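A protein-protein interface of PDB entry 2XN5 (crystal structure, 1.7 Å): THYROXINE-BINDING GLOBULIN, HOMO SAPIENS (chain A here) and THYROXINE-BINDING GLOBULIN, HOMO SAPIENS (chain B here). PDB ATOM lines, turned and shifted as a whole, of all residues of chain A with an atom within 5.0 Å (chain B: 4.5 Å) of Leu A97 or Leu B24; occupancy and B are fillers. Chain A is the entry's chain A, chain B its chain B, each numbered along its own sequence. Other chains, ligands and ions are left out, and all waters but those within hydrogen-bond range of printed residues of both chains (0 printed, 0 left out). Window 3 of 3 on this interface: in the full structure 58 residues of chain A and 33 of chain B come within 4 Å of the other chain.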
ATOM      1  N   PHE A  37     -30.839 -11.772  15.303  1.00  0.00           N
ATOM      2  CA  PHE A  37     -30.640 -11.335  16.683  1.00  0.00           C
ATOM      3  C   PHE A  37     -29.437 -11.978  17.359  1.00  0.00           C
ATOM      4  O   PHE A  37     -28.821 -12.904  16.826  1.00  0.00           O
ATOM      5  CB  PHE A  37     -31.908 -11.571  17.508  1.00  0.00           C
ATOM      6  CG  PHE A  37     -32.293 -13.013  17.666  1.00  0.00           C
ATOM      7  CD1 PHE A  37     -32.857 -13.720  16.610  1.00  0.00           C
ATOM      8  CD2 PHE A  37     -32.158 -13.651  18.892  1.00  0.00           C
ATOM      9  CE1 PHE A  37     -33.251 -15.046  16.768  1.00  0.00           C
ATOM     10  CE2 PHE A  37     -32.549 -14.980  19.050  1.00  0.00           C
ATOM     11  CZ  PHE A  37     -33.111 -15.669  17.979  1.00  0.00           C
ATOM     12  N   SER A  38     -29.077 -11.443  18.518  1.00  0.00           N
ATOM     13  CA  SER A  38     -28.067 -12.040  19.355  1.00  0.00           C
ATOM     14  C   SER A  38     -28.744 -12.721  20.542  1.00  0.00           C
ATOM     15  O   SER A  38     -29.139 -12.047  21.493  1.00  0.00           O
ATOM     16  CB  SER A  38     -27.078 -10.997  19.866  1.00  0.00           C
ATOM     17  OG  SER A  38     -26.167 -11.606  20.763  1.00  0.00           O
ATOM     18  N   PRO A  39     -28.870 -14.057  20.495  1.00  0.00           N
ATOM     19  CA  PRO A  39     -29.474 -14.770  21.629  1.00  0.00           C
ATOM     20  C   PRO A  39     -28.739 -14.561  22.943  1.00  0.00           C
ATOM     21  O   PRO A  39     -29.378 -14.376  23.977  1.00  0.00           O
ATOM     22  CB  PRO A  39     -29.386 -16.255  21.233  1.00  0.00           C
ATOM     23  CG  PRO A  39     -28.905 -16.302  19.825  1.00  0.00           C
ATOM     24  CD  PRO A  39     -28.464 -14.954  19.395  1.00  0.00           C
ATOM     25  N   VAL A  40     -27.410 -14.628  22.909  1.00  0.00           N
ATOM     26  CA  VAL A  40     -26.611 -14.453  24.115  1.00  0.00           C
ATOM     27  C   VAL A  40     -26.802 -13.058  24.733  1.00  0.00           C
ATOM     28  O   VAL A  40     -26.802 -12.928  25.953  1.00  0.00           O
ATOM     29  CB  VAL A  40     -25.103 -14.758  23.885  1.00  0.00           C
ATOM     30  CG1 VAL A  40     -24.451 -13.738  22.930  1.00  0.00           C
ATOM     31  CG2 VAL A  40     -24.373 -14.805  25.215  1.00  0.00           C
ATOM     32  N   LEU A  88     -15.980 -15.113  26.977  1.00  0.00           N
ATOM     33  CA  LEU A  88     -16.245 -14.448  25.693  1.00  0.00           C
ATOM     34  C   LEU A  88     -15.373 -13.207  25.519  1.00  0.00           C
ATOM     35  O   LEU A  88     -14.908 -12.924  24.414  1.00  0.00           O
ATOM     36  CB  LEU A  88     -17.732 -14.084  25.536  1.00  0.00           C
ATOM     37  CG  LEU A  88     -18.720 -15.248  25.381  1.00  0.00           C
ATOM     38  CD1 LEU A  88     -20.161 -14.727  25.343  1.00  0.00           C
ATOM     39  CD2 LEU A  88     -18.422 -16.115  24.156  1.00  0.00           C
ATOM     40  N   ASN A  89     -15.138 -12.492  26.618  1.00  0.00           N
ATOM     41  CA  ASN A  89     -14.342 -11.264  26.602  1.00  0.00           C
ATOM     42  C   ASN A  89     -12.828 -11.466  26.664  1.00  0.00           C
ATOM     43  O   ASN A  89     -12.075 -10.503  26.487  1.00  0.00           O
ATOM     44  CB  ASN A  89     -14.765 -10.351  27.758  1.00  0.00           C
ATOM     45  CG  ASN A  89     -16.077  -9.651  27.490  1.00  0.00           C
ATOM     46  OD1 ASN A  89     -16.369  -9.279  26.354  1.00  0.00           O
ATOM     47  ND2 ASN A  89     -16.866  -9.457  28.531  1.00  0.00           N
ATOM     48  N   LEU A  95      -9.377 -11.523  16.704  1.00  0.00           N
ATOM     49  CA  LEU A  95     -10.835 -11.559  16.825  1.00  0.00           C
ATOM     50  C   LEU A  95     -11.254 -10.441  17.775  1.00  0.00           C
ATOM     51  O   LEU A  95     -10.709 -10.325  18.876  1.00  0.00           O
ATOM     52  CB  LEU A  95     -11.329 -12.908  17.370  1.00  0.00           C
ATOM     53  CG  LEU A  95     -12.736 -12.919  17.994  1.00  0.00           C
ATOM     54  CD1 LEU A  95     -13.778 -12.632  16.933  1.00  0.00           C
ATOM     55  CD2 LEU A  95     -13.044 -14.233  18.703  1.00  0.00           C
ATOM     56  N   GLU A  96     -12.201  -9.617  17.336  1.00  0.00           N
ATOM     57  CA  GLU A  96     -12.835  -8.618  18.186  1.00  0.00           C
ATOM     58  C   GLU A  96     -14.127  -9.221  18.692  1.00  0.00           C
ATOM     59  O   GLU A  96     -15.019  -9.503  17.901  1.00  0.00           O
ATOM     60  CB  GLU A  96     -13.172  -7.344  17.404  1.00  0.00           C
ATOM     61  CG  GLU A  96     -12.281  -6.168  17.649  1.00  0.00           C
ATOM     62  CD  GLU A  96     -12.918  -4.875  17.184  1.00  0.00           C
ATOM     63  OE1 GLU A  96     -13.354  -4.081  18.045  1.00  0.00           O
ATOM     64  OE2 GLU A  96     -13.014  -4.666  15.960  1.00  0.00           O
ATOM     65  N   LEU A  97     -14.216  -9.449  19.995  1.00  0.00           N
ATOM     66  CA  LEU A  97     -15.471  -9.878  20.601  1.00  0.00           C
ATOM     67  C   LEU A  97     -15.598  -9.216  21.966  1.00  0.00           C
ATOM     68  O   LEU A  97     -14.776  -9.450  22.852  1.00  0.00           O
ATOM     69  CB  LEU A  97     -15.549 -11.404  20.695  1.00  0.00           C
ATOM     70  CG  LEU A  97     -16.776 -12.040  21.361  1.00  0.00           C
ATOM     71  CD1 LEU A  97     -18.089 -11.499  20.797  1.00  0.00           C
ATOM     72  CD2 LEU A  97     -16.720 -13.563  21.206  1.00  0.00           C
ATOM     73  N   GLN A  98     -16.602  -8.347  22.098  1.00  0.00           N
ATOM     74  CA  GLN A  98     -16.877  -7.628  23.348  1.00  0.00           C
ATOM     75  C   GLN A  98     -18.343  -7.851  23.704  1.00  0.00           C
ATOM     76  O   GLN A  98     -19.208  -7.640  22.868  1.00  0.00           O
ATOM     77  CB  GLN A  98     -16.626  -6.120  23.181  1.00  0.00           C
ATOM     78  CG  GLN A  98     -15.189  -5.710  22.790  1.00  0.00           C
ATOM     79  CD  GLN A  98     -15.007  -5.338  21.300  1.00  0.00           C
ATOM     80  OE1 GLN A  98     -15.939  -5.386  20.497  1.00  0.00           O
ATOM     81  NE2 GLN A  98     -13.783  -4.961  20.942  1.00  0.00           N
ATOM     82  N   ILE A  99     -18.618  -8.299  24.927  1.00  0.00           N
ATOM     83  CA  ILE A  99     -19.979  -8.339  25.450  1.00  0.00           C
ATOM     84  C   ILE A  99     -19.951  -7.715  26.842  1.00  0.00           C
ATOM     85  O   ILE A  99     -19.063  -8.002  27.643  1.00  0.00           O
ATOM     86  CB  ILE A  99     -20.563  -9.766  25.493  1.00  0.00           C
ATOM     87  CG1 ILE A  99     -22.029  -9.733  25.954  1.00  0.00           C
ATOM     88  CG2 ILE A  99     -19.732 -10.670  26.398  1.00  0.00           C
ATOM     89  CD1 ILE A  99     -22.771 -11.064  25.770  1.00  0.00           C
ATOM     90  N   ILE A 173     -23.261  -6.406  22.490  1.00  0.00           N
ATOM     91  CA  ILE A 173     -22.296  -7.345  21.943  1.00  0.00           C
ATOM     92  C   ILE A 173     -21.781  -6.786  20.612  1.00  0.00           C
ATOM     93  O   ILE A 173     -22.563  -6.288  19.791  1.00  0.00           O
ATOM     94  CB  ILE A 173     -22.914  -8.764  21.754  1.00  0.00           C
ATOM     95  CG1 ILE A 173     -21.860  -9.753  21.224  1.00  0.00           C
ATOM     96  CG2 ILE A 173     -24.149  -8.705  20.833  1.00  0.00           C
ATOM     97  CD1 ILE A 173     -22.284 -11.215  21.252  1.00  0.00           C
ATOM     98  N   HIS A 174     -20.463  -6.828  20.426  1.00  0.00           N
ATOM     99  CA  HIS A 174     -19.841  -6.472  19.154  1.00  0.00           C
ATOM    100  C   HIS A 174     -18.836  -7.562  18.762  1.00  0.00           C
ATOM    101  O   HIS A 174     -18.053  -8.041  19.597  1.00  0.00           O
ATOM    102  CB  HIS A 174     -19.164  -5.110  19.233  1.00  0.00           C
ATOM    103  CG  HIS A 174     -18.354  -4.776  18.017  1.00  0.00           C
ATOM    104  ND1 HIS A 174     -16.997  -4.979  17.956  1.00  0.00           N
ATOM    105  CD2 HIS A 174     -18.721  -4.313  16.803  1.00  0.00           C
ATOM    106  CE1 HIS A 174     -16.555  -4.629  16.760  1.00  0.00           C
ATOM    107  NE2 HIS A 174     -17.583  -4.224  16.041  1.00  0.00           N
ATOM    108  N   PHE A 175     -18.891  -7.941  17.491  1.00  0.00           N
ATOM    109  CA  PHE A 175     -18.116  -9.042  16.927  1.00  0.00           C
ATOM    110  C   PHE A 175     -17.564  -8.610  15.575  1.00  0.00           C
ATOM    111  O   PHE A 175     -18.316  -8.165  14.706  1.00  0.00           O
ATOM    112  CB  PHE A 175     -19.030 -10.262  16.740  1.00  0.00           C
ATOM    113  CG  PHE A 175     -18.394 -11.426  15.984  1.00  0.00           C
ATOM    114  CD1 PHE A 175     -17.577 -12.341  16.637  1.00  0.00           C
ATOM    115  CD2 PHE A 175     -18.654 -11.620  14.624  1.00  0.00           C
ATOM    116  CE1 PHE A 175     -16.996 -13.414  15.932  1.00  0.00           C
ATOM    117  CE2 PHE A 175     -18.081 -12.688  13.921  1.00  0.00           C
ATOM    118  CZ  PHE A 175     -17.265 -13.585  14.574  1.00  0.00           C
ATOM    119  N   ILE B  15     -23.727 -17.709  14.040  1.00  0.00           N
ATOM    120  CA  ILE B  15     -22.339 -17.410  14.360  1.00  0.00           C
ATOM    121  C   ILE B  15     -22.079 -17.970  15.754  1.00  0.00           C
ATOM    122  O   ILE B  15     -22.799 -17.645  16.702  1.00  0.00           O
ATOM    123  CB  ILE B  15     -22.065 -15.902  14.303  1.00  0.00           C
ATOM    124  CG1 ILE B  15     -22.263 -15.382  12.872  1.00  0.00           C
ATOM    125  CG2 ILE B  15     -20.642 -15.591  14.791  1.00  0.00           C
ATOM    126  CD1 ILE B  15     -22.145 -13.861  12.766  1.00  0.00           C
ATOM    127  N   LEU B  16     -21.081 -18.839  15.883  1.00  0.00           N
ATOM    128  CA  LEU B  16     -20.810 -19.441  17.180  1.00  0.00           C
ATOM    129  C   LEU B  16     -19.372 -19.277  17.612  1.00  0.00           C
ATOM    130  O   LEU B  16     -18.460 -19.118  16.775  1.00  0.00           O
ATOM    131  CB  LEU B  16     -21.293 -20.900  17.247  1.00  0.00           C
ATOM    132  CG  LEU B  16     -20.591 -22.086  16.618  1.00  0.00           C
ATOM    133  CD1 LEU B  16     -19.617 -22.737  17.612  1.00  0.00           C
ATOM    134  CD2 LEU B  16     -21.630 -23.138  16.106  1.00  0.00           C
ATOM    135  N   GLU B  17     -19.191 -19.231  18.928  1.00  0.00           N
ATOM    136  CA  GLU B  17     -17.875 -19.143  19.538  1.00  0.00           C
ATOM    137  C   GLU B  17     -17.556 -20.528  20.083  1.00  0.00           C
ATOM    138  O   GLU B  17     -18.341 -21.091  20.843  1.00  0.00           O
ATOM    139  CB  GLU B  17     -17.863 -18.082  20.636  1.00  0.00           C
ATOM    140  CG  GLU B  17     -16.480 -17.697  21.119  1.00  0.00           C
ATOM    141  CD  GLU B  17     -15.939 -18.602  22.225  1.00  0.00           C
ATOM    142  OE1 GLU B  17     -16.702 -19.402  22.792  1.00  0.00           O
ATOM    143  OE2 GLU B  17     -14.735 -18.496  22.534  1.00  0.00           O
ATOM    144  N   SER B  22     -21.101 -21.126  22.350  1.00  0.00           N
ATOM    145  CA  SER B  22     -22.193 -20.156  22.445  1.00  0.00           C
ATOM    146  C   SER B  22     -22.646 -19.687  21.068  1.00  0.00           C
ATOM    147  O   SER B  22     -21.819 -19.372  20.219  1.00  0.00           O
ATOM    148  CB  SER B  22     -21.750 -18.940  23.268  1.00  0.00           C
ATOM    149  OG  SER B  22     -22.764 -17.939  23.326  1.00  0.00           O
ATOM    150  N   ILE B  23     -23.962 -19.622  20.871  1.00  0.00           N
ATOM    151  CA  ILE B  23     -24.524 -18.971  19.693  1.00  0.00           C
ATOM    152  C   ILE B  23     -24.567 -17.467  19.958  1.00  0.00           C
ATOM    153  O   ILE B  23     -25.398 -16.987  20.743  1.00  0.00           O
ATOM    154  CB  ILE B  23     -25.949 -19.456  19.396  1.00  0.00           C
ATOM    155  CG1 ILE B  23     -25.976 -20.977  19.224  1.00  0.00           C
ATOM    156  CG2 ILE B  23     -26.487 -18.763  18.141  1.00  0.00           C
ATOM    157  CD1 ILE B  23     -27.349 -21.518  18.923  1.00  0.00           C
ATOM    158  N   LEU B  24     -23.672 -16.738  19.302  1.00  0.00           N
ATOM    159  CA  LEU B  24     -23.583 -15.295  19.439  1.00  0.00           C
ATOM    160  C   LEU B  24     -24.677 -14.584  18.641  1.00  0.00           C
ATOM    161  O   LEU B  24     -25.217 -13.583  19.105  1.00  0.00           O
ATOM    162  CB  LEU B  24     -22.206 -14.811  18.968  1.00  0.00           C
ATOM    163  CG  LEU B  24     -20.957 -15.426  19.607  1.00  0.00           C
ATOM    164  CD1 LEU B  24     -19.716 -14.797  18.983  1.00  0.00           C
ATOM    165  CD2 LEU B  24     -20.940 -15.252  21.118  1.00  0.00           C
ATOM    166  N   PHE B  25     -24.967 -15.093  17.437  1.00  0.00           N
ATOM    167  CA  PHE B  25     -25.973 -14.534  16.528  1.00  0.00           C
ATOM    168  C   PHE B  25     -26.671 -15.644  15.775  1.00  0.00           C
ATOM    169  O   PHE B  25     -26.059 -16.668  15.438  1.00  0.00           O
ATOM    170  CB  PHE B  25     -25.352 -13.576  15.502  1.00  0.00           C
ATOM    171  CG  PHE B  25     -24.659 -12.385  16.124  1.00  0.00           C
ATOM    172  CD1 PHE B  25     -25.359 -11.224  16.380  1.00  0.00           C
ATOM    173  CD2 PHE B  25     -23.310 -12.436  16.438  1.00  0.00           C
ATOM    174  CE1 PHE B  25     -24.725 -10.139  16.973  1.00  0.00           C
ATOM    175  CE2 PHE B  25     -22.673 -11.367  17.035  1.00  0.00           C
ATOM    176  CZ  PHE B  25     -23.378 -10.219  17.299  1.00  0.00           C
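O of Leu B24 lies within hydrogen-bond range of OG of Ser A38 (2.7 Å).
The backbone NH (N) of Glu B17 lies within hydrogen-bond range of the backbone carbonyl oxygen (O) of Ser B22 (2.9 Å).
The backbone carbonyl oxygen of Ile B15 is in hydrogen-bond range of the backbone NH of Leu B24.
The backbone carbonyl oxygen (O) of Phe B25 sits at hydrogen-bond distance from the backbone NH (N) of Ile B15, at 2.9 Å.
Among the printed residues, pairs that only touch across the chains: Phe A37 with Phe B25 (3.3 Å), Ser A38 with Phe B25 (3.8 Å), Pro A39 with Ile B23 (3.7 Å), Pro A39 with Leu B24 (3.5 Å), Pro A39 with Phe B25 (3.8 Å), Val A40 with Ser B22 (3.99 Å), Val A40 with Ile B23 (3.8 Å), Val A40 with Leu B24 (3.9 Å), Leu A88 with Glu B17 (3.9 Å), Leu A97 with Leu B24 (3.9 Å), Ile A173 with Phe B25 (3.9 Å), Phe A175 with Ile B15 (3.9 Å) and Phe A175 with Phe B25 (3.8 Å).
Leu A97 touches just one residue of chain B: Leu B24.
Of the printed residues of chain A, Leu B24 touches Ser A38, Pro A39, Val A40 and Leu A97.
Of the printed residues of chain A, Ile B15 touches Phe A175.
Of the printed residues of chain B, Phe A175 touches Ile B15 (3.9 Å) and Phe B25 (3.8 Å).
Printed residues of chain B within 4 Å of Ile A173: Phe B25.
Ile A99 touches none of the printed residues of chain B.
Of the 14 printed residues of chain A, 8 touch a printed residue of chain B.
Hydrophobic or aromatic side chains of chain A that line the printed part of chain B: Pro A39, Val A40, Leu A88, Leu A97, Ile A173 and Phe A175.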
